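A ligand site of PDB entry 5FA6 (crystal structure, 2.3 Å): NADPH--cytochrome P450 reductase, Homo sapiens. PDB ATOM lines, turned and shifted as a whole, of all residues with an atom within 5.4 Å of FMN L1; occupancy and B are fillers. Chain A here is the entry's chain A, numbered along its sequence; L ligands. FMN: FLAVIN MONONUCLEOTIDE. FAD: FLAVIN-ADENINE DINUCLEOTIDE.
The side-chain hydroxyl (OG) of Ser 27 lies within hydrogen-bond range of the backbone NH (N) of Gly 30 (2.9 Å).
OG1 of Thr 87 is in hydrogen-bond range of N of Ser 27 (3.2 Å).
OD1 of Asn 123 sits at hydrogen-bond distance from N of Gly 115 (3.1 Å).
The side-chain amide oxygen (OD1) of Asn 123 sits close to the backbone NH (N) of Leu 114, at 3.2 Å.
The backbone NH of Thr 80 sits at hydrogen-bond distance from the backbone carbonyl oxygen of Leu 114 (3.0 Å).
The backbone NH (N) of Ala 124 is in hydrogen-bond range of the side-chain hydroxyl (OG1) of Thr 80 (3.4 Å).
The backbone NH (N) of Asp 149 sits at hydrogen-bond distance from the backbone carbonyl oxygen (O) of Gly 115.
N of Ala 79 is in hydrogen-bond range of O of Gly 26 (3.2 Å).
N of Thr 29 lies within hydrogen-bond range of O2P of FMN L1, 3.1 Å away.
The side-chain hydroxyl (OG1) of Thr 29 is in hydrogen-bond range of an oxygen (O1P) of FMN L1 (2.4 Å).
An oxygen (O3P) of FMN L1 lies within hydrogen-bond range of the side-chain hydroxyl of Ser 27.
The backbone NH (N) of Ala 32 is in hydrogen-bond range of an oxygen (O3P) of FMN L1 (2.5 Å).
The backbone NH of Gln 28 sits at hydrogen-bond distance from an oxygen (O2P) of FMN L1 (2.6 Å).
O of Tyr 81 lies close to O4 of FMN L1 (2.6 Å).
OH of Tyr 81 sits at hydrogen-bond distance from O2P of FMN L1 (3.0 Å).
The backbone NH (N) of Thr 31 is in hydrogen-bond range of an oxygen (O1P) of FMN L1 (2.9 Å).
An oxygen (O1P) of FMN L1 sits at hydrogen-bond distance from the side-chain hydroxyl of Thr 31, 2.8 Å away.
N of Asn 123 is in hydrogen-bond range of O2 of FMN L1, 2.8 Å away.
N of Asn 116 sits at hydrogen-bond distance from O2 of FMN L1 (2.8 Å).
N of Thr 80 lies within hydrogen-bond range of O2' of FMN L1 (3.4 Å).
O of Thr 80 sits at hydrogen-bond distance from O2' of FMN L1.
The backbone carbonyl oxygen (O) of His 121 sits at hydrogen-bond distance from a nitrogen (N3) of FMN L1 (3.1 Å).
O of Leu 114 is in hydrogen-bond range of O2' of FMN L1, 3.2 Å away.
N of Gly 30 sits at hydrogen-bond distance from O1P of FMN L1 (3.3 Å).
The side-chain carboxylate of Asp 149 is in hydrogen-bond range of an oxygen (O3') of FMN L1 (3.3 Å).
The backbone NH of Gly 84 sits at hydrogen-bond distance from an oxygen (O4) of FMN L1.
Merely in contact with FMN L1: Ala 79 (3.3 Å), Gly 82 (3.9 Å), Gly 115 (3.2 Å), Tyr 119 (3.5 Å), Phe 122 (3.5 Å) and Leu 153 (3.5 Å).
Hydrophobic or aromatic side chains within 4 Å of FMN L1: Ala 32, Ala 79, Tyr 81, Leu 114, Tyr 119, Phe 122 and Leu 153.
20 residues have an atom within 4 Å of FMN L1: Ser 27, Gln 28, Thr 29, Gly 30, Thr 31, Ala 32, Ala 79, Thr 80, Tyr 81, Gly 82, Gly 84, Leu 114, Gly 115, Asn 116, Tyr 119, His 121, Phe 122, Asn 123, Asp 149 and Leu 153.
The nearest printed residue that does not touch FMN L1 is Glu 83 (4.03 Å).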
ATOM      1  N   GLY A  26       7.556  18.017  -5.072  1.00  0.00           N
ATOM      2  CA  GLY A  26       6.821  17.420  -3.969  1.00  0.00           C
ATOM      3  C   GLY A  26       5.795  18.532  -3.830  1.00  0.00           C
ATOM      4  O   GLY A  26       6.129  19.641  -3.396  1.00  0.00           O
ATOM      5  N   SER A  27       4.551  18.249  -4.185  1.00  0.00           N
ATOM      6  CA  SER A  27       3.549  19.295  -4.167  1.00  0.00           C
ATOM      7  C   SER A  27       2.168  18.835  -3.798  1.00  0.00           C
ATOM      8  O   SER A  27       1.732  17.743  -4.155  1.00  0.00           O
ATOM      9  CB  SER A  27       3.481  20.070  -5.494  1.00  0.00           C
ATOM     10  OG  SER A  27       2.640  21.202  -5.388  1.00  0.00           O
ATOM     11  N   GLN A  28       1.461  19.700  -3.066  1.00  0.00           N
ATOM     12  CA  GLN A  28       0.105  19.390  -2.703  1.00  0.00           C
ATOM     13  C   GLN A  28      -0.844  20.381  -3.368  1.00  0.00           C
ATOM     14  O   GLN A  28      -1.870  19.971  -3.899  1.00  0.00           O
ATOM     15  CB  GLN A  28      -0.081  19.400  -1.183  1.00  0.00           C
ATOM     16  CG  GLN A  28      -1.401  18.755  -0.787  1.00  0.00           C
ATOM     17  CD  GLN A  28      -1.493  18.408   0.692  1.00  0.00           C
ATOM     18  OE1 GLN A  28      -0.642  17.694   1.221  1.00  0.00           O
ATOM     19  NE2 GLN A  28      -2.537  18.903   1.356  1.00  0.00           N
ATOM     20  N   THR A  29      -0.497  21.669  -3.368  1.00  0.00           N
ATOM     21  CA  THR A  29      -1.344  22.685  -3.997  1.00  0.00           C
ATOM     22  C   THR A  29      -0.746  23.346  -5.257  1.00  0.00           C
ATOM     23  O   THR A  29      -1.039  24.518  -5.572  1.00  0.00           O
ATOM     24  CB  THR A  29      -1.797  23.791  -2.984  1.00  0.00           C
ATOM     25  OG1 THR A  29      -0.654  24.522  -2.528  1.00  0.00           O
ATOM     26  CG2 THR A  29      -2.522  23.158  -1.781  1.00  0.00           C
ATOM     27  N   GLY A  30       0.099  22.579  -5.952  1.00  0.00           N
ATOM     28  CA  GLY A  30       0.697  23.010  -7.210  1.00  0.00           C
ATOM     29  C   GLY A  30       1.869  23.974  -7.285  1.00  0.00           C
ATOM     30  O   GLY A  30       2.475  24.102  -8.350  1.00  0.00           O
ATOM     31  N   THR A  31       2.202  24.648  -6.183  1.00  0.00           N
ATOM     32  CA  THR A  31       3.293  25.622  -6.170  1.00  0.00           C
ATOM     33  C   THR A  31       4.664  25.002  -6.495  1.00  0.00           C
ATOM     34  O   THR A  31       5.412  25.504  -7.340  1.00  0.00           O
ATOM     35  CB  THR A  31       3.419  26.325  -4.798  1.00  0.00           C
ATOM     36  OG1 THR A  31       2.104  26.604  -4.276  1.00  0.00           O
ATOM     37  CG2 THR A  31       4.207  27.631  -4.926  1.00  0.00           C
ATOM     38  N   ALA A  32       4.991  23.915  -5.811  1.00  0.00           N
ATOM     39  CA  ALA A  32       6.257  23.260  -6.067  1.00  0.00           C
ATOM     40  C   ALA A  32       6.260  22.800  -7.517  1.00  0.00           C
ATOM     41  O   ALA A  32       7.283  22.870  -8.196  1.00  0.00           O
ATOM     42  CB  ALA A  32       6.448  22.057  -5.096  1.00  0.00           C
ATOM     43  N   GLU A  33       5.109  22.335  -8.013  1.00  0.00           N
ATOM     44  CA  GLU A  33       5.022  21.877  -9.383  1.00  0.00           C
ATOM     45  C   GLU A  33       5.334  23.000 -10.372  1.00  0.00           C
ATOM     46  O   GLU A  33       6.198  22.847 -11.242  1.00  0.00           O
ATOM     47  CB  GLU A  33       3.646  21.283  -9.695  1.00  0.00           C
ATOM     48  CG  GLU A  33       3.509  20.942 -11.170  1.00  0.00           C
ATOM     49  CD  GLU A  33       2.253  20.171 -11.493  1.00  0.00           C
ATOM     50  OE1 GLU A  33       2.052  19.883 -12.696  1.00  0.00           O
ATOM     51  OE2 GLU A  33       1.475  19.843 -10.571  1.00  0.00           O
ATOM     52  N   ALA A  79       7.834  20.826  -0.954  1.00  0.00           N
ATOM     53  CA  ALA A  79       7.088  21.595   0.010  1.00  0.00           C
ATOM     54  C   ALA A  79       6.920  20.720   1.248  1.00  0.00           C
ATOM     55  O   ALA A  79       7.017  19.496   1.161  1.00  0.00           O
ATOM     56  CB  ALA A  79       5.742  21.983  -0.572  1.00  0.00           C
ATOM     57  N   THR A  80       6.698  21.336   2.394  1.00  0.00           N
ATOM     58  CA  THR A  80       6.495  20.595   3.635  1.00  0.00           C
ATOM     59  C   THR A  80       5.044  20.683   4.142  1.00  0.00           C
ATOM     60  O   THR A  80       4.384  21.706   3.968  1.00  0.00           O
ATOM     61  CB  THR A  80       7.415  21.132   4.765  1.00  0.00           C
ATOM     62  OG1 THR A  80       8.785  21.052   4.336  1.00  0.00           O
ATOM     63  CG2 THR A  80       7.247  20.286   6.027  1.00  0.00           C
ATOM     64  N   TYR A  81       4.559  19.610   4.744  1.00  0.00           N
ATOM     65  CA  TYR A  81       3.203  19.597   5.286  1.00  0.00           C
ATOM     66  C   TYR A  81       3.030  19.343   6.773  1.00  0.00           C
ATOM     67  O   TYR A  81       3.841  19.812   7.568  1.00  0.00           O
ATOM     68  CB  TYR A  81       2.250  18.797   4.385  1.00  0.00           C
ATOM     69  CG  TYR A  81       1.709  19.657   3.269  1.00  0.00           C
ATOM     70  CD1 TYR A  81       2.478  19.917   2.127  1.00  0.00           C
ATOM     71  CD2 TYR A  81       0.476  20.287   3.393  1.00  0.00           C
ATOM     72  CE1 TYR A  81       2.028  20.798   1.141  1.00  0.00           C
ATOM     73  CE2 TYR A  81       0.019  21.174   2.396  1.00  0.00           C
ATOM     74  CZ  TYR A  81       0.801  21.423   1.277  1.00  0.00           C
ATOM     75  OH  TYR A  81       0.371  22.297   0.311  1.00  0.00           O
ATOM     76  N   GLY A  82       1.975  18.626   7.129  1.00  0.00           N
ATOM     77  CA  GLY A  82       1.717  18.237   8.511  1.00  0.00           C
ATOM     78  C   GLY A  82       2.995  17.868   9.260  1.00  0.00           C
ATOM     79  O   GLY A  82       3.669  16.886   8.898  1.00  0.00           O
ATOM     80  N   GLU A  83       3.321  18.626  10.301  1.00  0.00           N
ATOM     81  CA  GLU A  83       4.505  18.377  11.124  1.00  0.00           C
ATOM     82  C   GLU A  83       5.874  18.063  10.533  1.00  0.00           C
ATOM     83  O   GLU A  83       6.586  17.207  11.065  1.00  0.00           O
ATOM     84  CB  GLU A  83       4.128  17.259  12.108  1.00  0.00           C
ATOM     85  CG  GLU A  83       3.027  17.598  13.080  1.00  0.00           C
ATOM     86  CD  GLU A  83       1.909  16.567  13.052  1.00  0.00           C
ATOM     87  OE1 GLU A  83       1.073  16.640  12.113  1.00  0.00           O
ATOM     88  OE2 GLU A  83       1.879  15.692  13.957  1.00  0.00           O
ATOM     89  N   GLY A  84       6.232  18.752   9.454  1.00  0.00           N
ATOM     90  CA  GLY A  84       7.529  18.507   8.843  1.00  0.00           C
ATOM     91  C   GLY A  84       7.482  17.184   8.091  1.00  0.00           C
ATOM     92  O   GLY A  84       8.429  16.411   8.109  1.00  0.00           O
ATOM     93  N   ASP A  85       6.355  16.929   7.441  1.00  0.00           N
ATOM     94  CA  ASP A  85       6.143  15.712   6.680  1.00  0.00           C
ATOM     95  C   ASP A  85       6.134  15.972   5.158  1.00  0.00           C
ATOM     96  O   ASP A  85       5.898  17.098   4.704  1.00  0.00           O
ATOM     97  CB  ASP A  85       4.781  15.109   7.060  1.00  0.00           C
ATOM     98  CG  ASP A  85       4.903  14.035   8.131  1.00  0.00           C
ATOM     99  OD1 ASP A  85       5.672  14.214   9.100  1.00  0.00           O
ATOM    100  OD2 ASP A  85       4.208  13.005   8.011  1.00  0.00           O
ATOM    101  N   THR A  87       4.834  15.899   1.226  1.00  0.00           N
ATOM    102  CA  THR A  87       3.547  15.982   0.544  1.00  0.00           C
ATOM    103  C   THR A  87       3.240  14.524   0.167  1.00  0.00           C
ATOM    104  O   THR A  87       4.170  13.695   0.065  1.00  0.00           O
ATOM    105  CB  THR A  87       3.644  16.839  -0.735  1.00  0.00           C
ATOM    106  OG1 THR A  87       4.634  16.272  -1.614  1.00  0.00           O
ATOM    107  CG2 THR A  87       4.070  18.252  -0.379  1.00  0.00           C
ATOM    108  N   LEU A 114      10.101  24.416  -0.232  1.00  0.00           N
ATOM    109  CA  LEU A 114       8.959  25.314  -0.033  1.00  0.00           C
ATOM    110  C   LEU A 114       8.408  25.072   1.362  1.00  0.00           C
ATOM    111  O   LEU A 114       7.953  23.960   1.682  1.00  0.00           O
ATOM    112  CB  LEU A 114       7.838  25.061  -1.055  1.00  0.00           C
ATOM    113  CG  LEU A 114       8.040  25.537  -2.493  1.00  0.00           C
ATOM    114  CD1 LEU A 114       8.934  24.541  -3.233  1.00  0.00           C
ATOM    115  CD2 LEU A 114       6.674  25.654  -3.165  1.00  0.00           C
ATOM    116  N   GLY A 115       8.453  26.105   2.202  1.00  0.00           N
ATOM    117  CA  GLY A 115       7.952  25.999   3.561  1.00  0.00           C
ATOM    118  C   GLY A 115       7.321  27.274   4.120  1.00  0.00           C
ATOM    119  O   GLY A 115       7.134  28.253   3.386  1.00  0.00           O
ATOM    120  N   ASN A 116       7.011  27.260   5.409  1.00  0.00           N
ATOM    121  CA  ASN A 116       6.384  28.408   6.058  1.00  0.00           C
ATOM    122  C   ASN A 116       6.904  28.547   7.492  1.00  0.00           C
ATOM    123  O   ASN A 116       6.685  27.651   8.307  1.00  0.00           O
ATOM    124  CB  ASN A 116       4.867  28.224   6.078  1.00  0.00           C
ATOM    125  CG  ASN A 116       4.127  29.429   6.652  1.00  0.00           C
ATOM    126  OD1 ASN A 116       4.591  30.069   7.605  1.00  0.00           O
ATOM    127  ND2 ASN A 116       2.950  29.726   6.086  1.00  0.00           N
ATOM    128  N   LYS A 117       7.552  29.662   7.793  1.00  0.00           N
ATOM    129  CA  LYS A 117       8.105  29.903   9.128  1.00  0.00           C
ATOM    130  C   LYS A 117       7.094  29.825  10.292  1.00  0.00           C
ATOM    131  O   LYS A 117       7.467  29.486  11.417  1.00  0.00           O
ATOM    132  CB  LYS A 117       8.811  31.268   9.170  1.00  0.00           C
ATOM    133  CG  LYS A 117      10.117  31.300   8.361  1.00  0.00           C
ATOM    134  CD  LYS A 117      11.000  32.477   8.748  1.00  0.00           C
ATOM    135  CE  LYS A 117      12.324  32.490   7.972  1.00  0.00           C
ATOM    136  NZ  LYS A 117      12.224  33.037   6.567  1.00  0.00           N
ATOM    137  N   TYR A 119       5.085  27.649  10.889  1.00  0.00           N
ATOM    138  CA  TYR A 119       4.901  26.241  11.262  1.00  0.00           C
ATOM    139  C   TYR A 119       6.074  25.736  12.124  1.00  0.00           C
ATOM    140  O   TYR A 119       7.184  26.256  12.034  1.00  0.00           O
ATOM    141  CB  TYR A 119       4.747  25.390   9.989  1.00  0.00           C
ATOM    142  CG  TYR A 119       3.380  25.497   9.339  1.00  0.00           C
ATOM    143  CD1 TYR A 119       2.310  24.723   9.783  1.00  0.00           C
ATOM    144  CD2 TYR A 119       3.143  26.402   8.298  1.00  0.00           C
ATOM    145  CE1 TYR A 119       1.032  24.854   9.213  1.00  0.00           C
ATOM    146  CE2 TYR A 119       1.873  26.538   7.725  1.00  0.00           C
ATOM    147  CZ  TYR A 119       0.823  25.757   8.189  1.00  0.00           C
ATOM    148  OH  TYR A 119      -0.439  25.890   7.638  1.00  0.00           O
ATOM    149  N   GLU A 120       5.810  24.731  12.968  1.00  0.00           N
ATOM    150  CA  GLU A 120       6.841  24.171  13.846  1.00  0.00           C
ATOM    151  C   GLU A 120       8.115  23.747  13.124  1.00  0.00           C
ATOM    152  O   GLU A 120       9.182  24.353  13.286  1.00  0.00           O
ATOM    153  CB  GLU A 120       6.296  22.954  14.621  1.00  0.00           C
ATOM    154  CG  GLU A 120       5.835  23.250  16.048  1.00  0.00           C
ATOM    155  CD  GLU A 120       6.953  23.817  16.926  1.00  0.00           C
ATOM    156  OE1 GLU A 120       7.965  23.098  17.152  1.00  0.00           O
ATOM    157  OE2 GLU A 120       6.827  24.974  17.372  1.00  0.00           O
ATOM    158  N   HIS A 121       7.994  22.692  12.317  1.00  0.00           N
ATOM    159  CA  HIS A 121       9.118  22.151  11.564  1.00  0.00           C
ATOM    160  C   HIS A 121       9.253  22.863  10.212  1.00  0.00           C
ATOM    161  O   HIS A 121       8.696  22.407   9.205  1.00  0.00           O
ATOM    162  CB  HIS A 121       8.903  20.648  11.353  1.00  0.00           C
ATOM    163  CG  HIS A 121       8.631  19.888  12.605  1.00  0.00           C
ATOM    164  ND1 HIS A 121       9.578  19.716  13.597  1.00  0.00           N
ATOM    165  CD2 HIS A 121       7.528  19.207  13.010  1.00  0.00           C
ATOM    166  CE1 HIS A 121       9.068  18.955  14.562  1.00  0.00           C
ATOM    167  NE2 HIS A 121       7.831  18.631  14.227  1.00  0.00           N
ATOM    168  N   PHE A 122       9.987  23.970  10.197  1.00  0.00           N
ATOM    169  CA  PHE A 122      10.180  24.758   8.988  1.00  0.00           C
ATOM    170  C   PHE A 122      10.997  24.106   7.866  1.00  0.00           C
ATOM    171  O   PHE A 122      12.166  23.786   8.037  1.00  0.00           O
ATOM    172  CB  PHE A 122      10.821  26.093   9.331  1.00  0.00           C
ATOM    173  CG  PHE A 122      11.144  26.944   8.125  1.00  0.00           C
ATOM    174  CD1 PHE A 122      10.141  27.301   7.230  1.00  0.00           C
ATOM    175  CD2 PHE A 122      12.439  27.408   7.908  1.00  0.00           C
ATOM    176  CE1 PHE A 122      10.415  28.138   6.135  1.00  0.00           C
ATOM    177  CE2 PHE A 122      12.719  28.236   6.814  1.00  0.00           C
ATOM    178  CZ  PHE A 122      11.712  28.606   5.937  1.00  0.00           C
ATOM    179  N   ASN A 123      10.361  23.948   6.705  1.00  0.00           N
ATOM    180  CA  ASN A 123      11.008  23.392   5.526  1.00  0.00           C
ATOM    181  C   ASN A 123      11.688  22.074   5.818  1.00  0.00           C
ATOM    182  O   ASN A 123      12.691  21.746   5.223  1.00  0.00           O
ATOM    183  CB  ASN A 123      12.043  24.391   4.972  1.00  0.00           C
ATOM    184  CG  ASN A 123      11.558  25.132   3.723  1.00  0.00           C
ATOM    185  OD1 ASN A 123      10.992  24.515   2.805  1.00  0.00           O
ATOM    186  ND2 ASN A 123      11.760  26.461   3.676  1.00  0.00           N
ATOM    187  N   ALA A 124      11.130  21.326   6.764  1.00  0.00           N
ATOM    188  CA  ALA A 124      11.707  20.051   7.138  1.00  0.00           C
ATOM    189  C   ALA A 124      11.914  19.078   5.952  1.00  0.00           C
ATOM    190  O   ALA A 124      12.875  18.311   5.946  1.00  0.00           O
ATOM    191  CB  ALA A 124      10.848  19.393   8.225  1.00  0.00           C
ATOM    192  N   ASP A 149       6.796  30.946   2.693  1.00  0.00           N
ATOM    193  CA  ASP A 149       5.516  31.445   2.224  1.00  0.00           C
ATOM    194  C   ASP A 149       4.895  32.491   3.184  1.00  0.00           C
ATOM    195  O   ASP A 149       3.880  33.116   2.846  1.00  0.00           O
ATOM    196  CB  ASP A 149       4.565  30.254   2.021  1.00  0.00           C
ATOM    197  CG  ASP A 149       3.324  30.600   1.212  1.00  0.00           C
ATOM    198  OD1 ASP A 149       3.423  31.347   0.206  1.00  0.00           O
ATOM    199  OD2 ASP A 149       2.229  30.098   1.564  1.00  0.00           O
ATOM    200  N   LEU A 153       7.266  33.741  -0.963  1.00  0.00           N
ATOM    201  CA  LEU A 153       7.832  32.538  -1.553  1.00  0.00           C
ATOM    202  C   LEU A 153       8.339  32.847  -2.960  1.00  0.00           C
ATOM    203  O   LEU A 153       9.452  32.473  -3.318  1.00  0.00           O
ATOM    204  CB  LEU A 153       6.757  31.446  -1.613  1.00  0.00           C
ATOM    205  CG  LEU A 153       7.185  30.065  -2.138  1.00  0.00           C
ATOM    206  CD1 LEU A 153       8.175  29.461  -1.143  1.00  0.00           C
ATOM    207  CD2 LEU A 153       5.974  29.166  -2.312  1.00  0.00           C
HETATM  208  N1  FMN L   1       5.566  24.695   5.785  1.00  0.00           N
HETATM  209  C2  FMN L   1       6.599  24.293   6.585  1.00  0.00           C
HETATM  210  O2  FMN L   1       7.723  24.775   6.503  1.00  0.00           O
HETATM  211  N3  FMN L   1       6.313  23.301   7.521  1.00  0.00           N
HETATM  212  C4  FMN L   1       5.079  22.683   7.738  1.00  0.00           C
HETATM  213  O4  FMN L   1       5.083  21.837   8.613  1.00  0.00           O
HETATM  214  C4A FMN L   1       3.997  23.097   6.919  1.00  0.00           C
HETATM  215  N5  FMN L   1       2.754  22.474   7.138  1.00  0.00           N
HETATM  216  C5A FMN L   1       1.722  22.920   6.307  1.00  0.00           C
HETATM  217  C6  FMN L   1       0.437  22.306   6.527  1.00  0.00           C
HETATM  218  C7  FMN L   1      -0.710  22.675   5.766  1.00  0.00           C
HETATM  219  C7M FMN L   1      -2.022  21.941   6.110  1.00  0.00           C
HETATM  220  C8  FMN L   1      -0.594  23.713   4.692  1.00  0.00           C
HETATM  221  C8M FMN L   1      -1.628  24.148   3.874  1.00  0.00           C
HETATM  222  C9  FMN L   1       0.636  24.313   4.459  1.00  0.00           C
HETATM  223  C9A FMN L   1       1.829  23.944   5.257  1.00  0.00           C
HETATM  224  N10 FMN L   1       3.177  24.547   5.074  1.00  0.00           N
HETATM  225  C10 FMN L   1       4.308  24.113   5.945  1.00  0.00           C
HETATM  226  C1' FMN L   1       3.355  25.560   4.041  1.00  0.00           C
HETATM  227  C2' FMN L   1       3.643  24.968   2.625  1.00  0.00           C
HETATM  228  O2' FMN L   1       4.890  24.162   2.705  1.00  0.00           O
HETATM  229  C3' FMN L   1       3.785  26.080   1.603  1.00  0.00           C
HETATM  230  O3' FMN L   1       2.518  26.785   1.580  1.00  0.00           O
HETATM  231  C4' FMN L   1       4.115  25.455   0.181  1.00  0.00           C
HETATM  232  O4' FMN L   1       4.240  26.677  -0.628  1.00  0.00           O
HETATM  233  C5' FMN L   1       2.997  24.646  -0.476  1.00  0.00           C
HETATM  234  O5' FMN L   1       3.454  24.076  -1.778  1.00  0.00           O
HETATM  235  P   FMN L   1       2.603  23.204  -2.796  1.00  0.00           P
HETATM  236  O1P FMN L   1       1.550  24.037  -3.405  1.00  0.00           O
HETATM  237  O2P FMN L   1       2.212  21.925  -1.990  1.00  0.00           O
HETATM  238  O3P FMN L   1       3.696  22.893  -3.929  1.00  0.00           O
HETATM  239  PA  FAD L   2      -9.007  33.093  -1.209  1.00  0.00           P
HETATM  240  O1A FAD L   2      -9.656  33.517  -2.462  1.00  0.00           O
HETATM  241  O2A FAD L   2      -8.266  31.808  -1.178  1.00  0.00           O
HETATM  242  O5B FAD L   2      -8.040  34.262  -0.693  1.00  0.00           O
HETATM  243  C5B FAD L   2      -7.366  34.121   0.554  1.00  0.00           C
HETATM  244  C4B FAD L   2      -6.283  35.196   0.699  1.00  0.00           C
HETATM  245  O4B FAD L   2      -6.842  36.518   0.673  1.00  0.00           O
HETATM  246  C3B FAD L   2      -5.656  35.144   2.085  1.00  0.00           C
HETATM  247  O3B FAD L   2      -4.725  34.053   2.157  1.00  0.00           O
HETATM  248  C2B FAD L   2      -4.887  36.448   2.022  1.00  0.00           C
HETATM  249  O2B FAD L   2      -3.678  36.263   1.250  1.00  0.00           O
HETATM  250  C1B FAD L   2      -5.846  37.372   1.290  1.00  0.00           C
HETATM  251  N9A FAD L   2      -6.556  38.248   2.237  1.00  0.00           N
HETATM  252  C8A FAD L   2      -7.576  37.829   3.222  1.00  0.00           C
HETATM  253  N7A FAD L   2      -7.818  39.098   3.931  1.00  0.00           N
HETATM  254  C5A FAD L   2      -7.097  40.053   3.355  1.00  0.00           C
HETATM  255  C6A FAD L   2      -7.012  41.341   3.668  1.00  0.00           C
HETATM  256  N6A FAD L   2      -8.040  41.837   4.350  1.00  0.00           N
HETATM  257  N1A FAD L   2      -6.046  42.137   3.198  1.00  0.00           N
HETATM  258  C2A FAD L   2      -5.106  41.607   2.305  1.00  0.00           C
HETATM  259  N3A FAD L   2      -5.244  40.255   1.960  1.00  0.00           N
HETATM  260  C4A FAD L   2      -6.231  39.515   2.491  1.00  0.00           C
HETATM  261  N1  FAD L   2     -10.846  28.812   7.349  1.00  0.00           N
HETATM  262  C2  FAD L   2     -12.071  28.873   8.027  1.00  0.00           C
HETATM  263  O2  FAD L   2     -12.797  29.850   7.910  1.00  0.00           O
HETATM  264  N3  FAD L   2     -12.499  27.766   8.775  1.00  0.00           N
HETATM  265  C4  FAD L   2     -11.702  26.625   8.861  1.00  0.00           C
HETATM  266  O4  FAD L   2     -12.095  25.660   9.522  1.00  0.00           O
HETATM  267  C4X FAD L   2     -10.490  26.568   8.184  1.00  0.00           C
HETATM  268  N5  FAD L   2      -9.625  25.573   8.436  1.00  0.00           N
HETATM  269  C5X FAD L   2      -8.472  25.514   7.764  1.00  0.00           C
HETATM  270  C6  FAD L   2      -7.633  24.414   7.929  1.00  0.00           C
HETATM  271  C7  FAD L   2      -6.525  24.241   7.124  1.00  0.00           C
HETATM  272  C7M FAD L   2      -5.751  23.089   7.235  1.00  0.00           C
HETATM  273  C8  FAD L   2      -6.227  25.198   6.143  1.00  0.00           C
HETATM  274  C8M FAD L   2      -5.182  24.982   5.261  1.00  0.00           C
HETATM  275  C9  FAD L   2      -7.046  26.315   6.003  1.00  0.00           C
HETATM  276  C9A FAD L   2      -8.172  26.475   6.804  1.00  0.00           C
HETATM  277  N10 FAD L   2      -9.025  27.484   6.589  1.00  0.00           N
HETATM  278  C10 FAD L   2     -10.061  27.650   7.430  1.00  0.00           C
HETATM  279  C1' FAD L   2      -8.747  28.520   5.582  1.00  0.00           C
HETATM  280  C2' FAD L   2      -9.485  28.184   4.275  1.00  0.00           C
HETATM  281  O2' FAD L   2      -9.042  26.936   3.759  1.00  0.00           O
HETATM  282  C3' FAD L   2      -9.305  29.281   3.222  1.00  0.00           C
HETATM  283  O3' FAD L   2      -7.922  29.634   3.083  1.00  0.00           O
HETATM  284  C4' FAD L   2     -10.110  30.513   3.642  1.00  0.00           C
HETATM  285  O4' FAD L   2     -11.459  30.129   3.898  1.00  0.00           O
HETATM  286  C5' FAD L   2     -10.060  31.560   2.520  1.00  0.00           C
HETATM  287  O5' FAD L   2     -10.442  30.916   1.292  1.00  0.00           O
HETATM  288  P   FAD L   2     -11.112  31.761   0.098  1.00  0.00           P
HETATM  289  O1P FAD L   2     -12.435  32.250   0.532  1.00  0.00           O
HETATM  290  O2P FAD L   2     -11.036  30.926  -1.128  1.00  0.00           O
HETATM  291  O3P FAD L   2     -10.137  33.031  -0.048  1.00  0.00           O
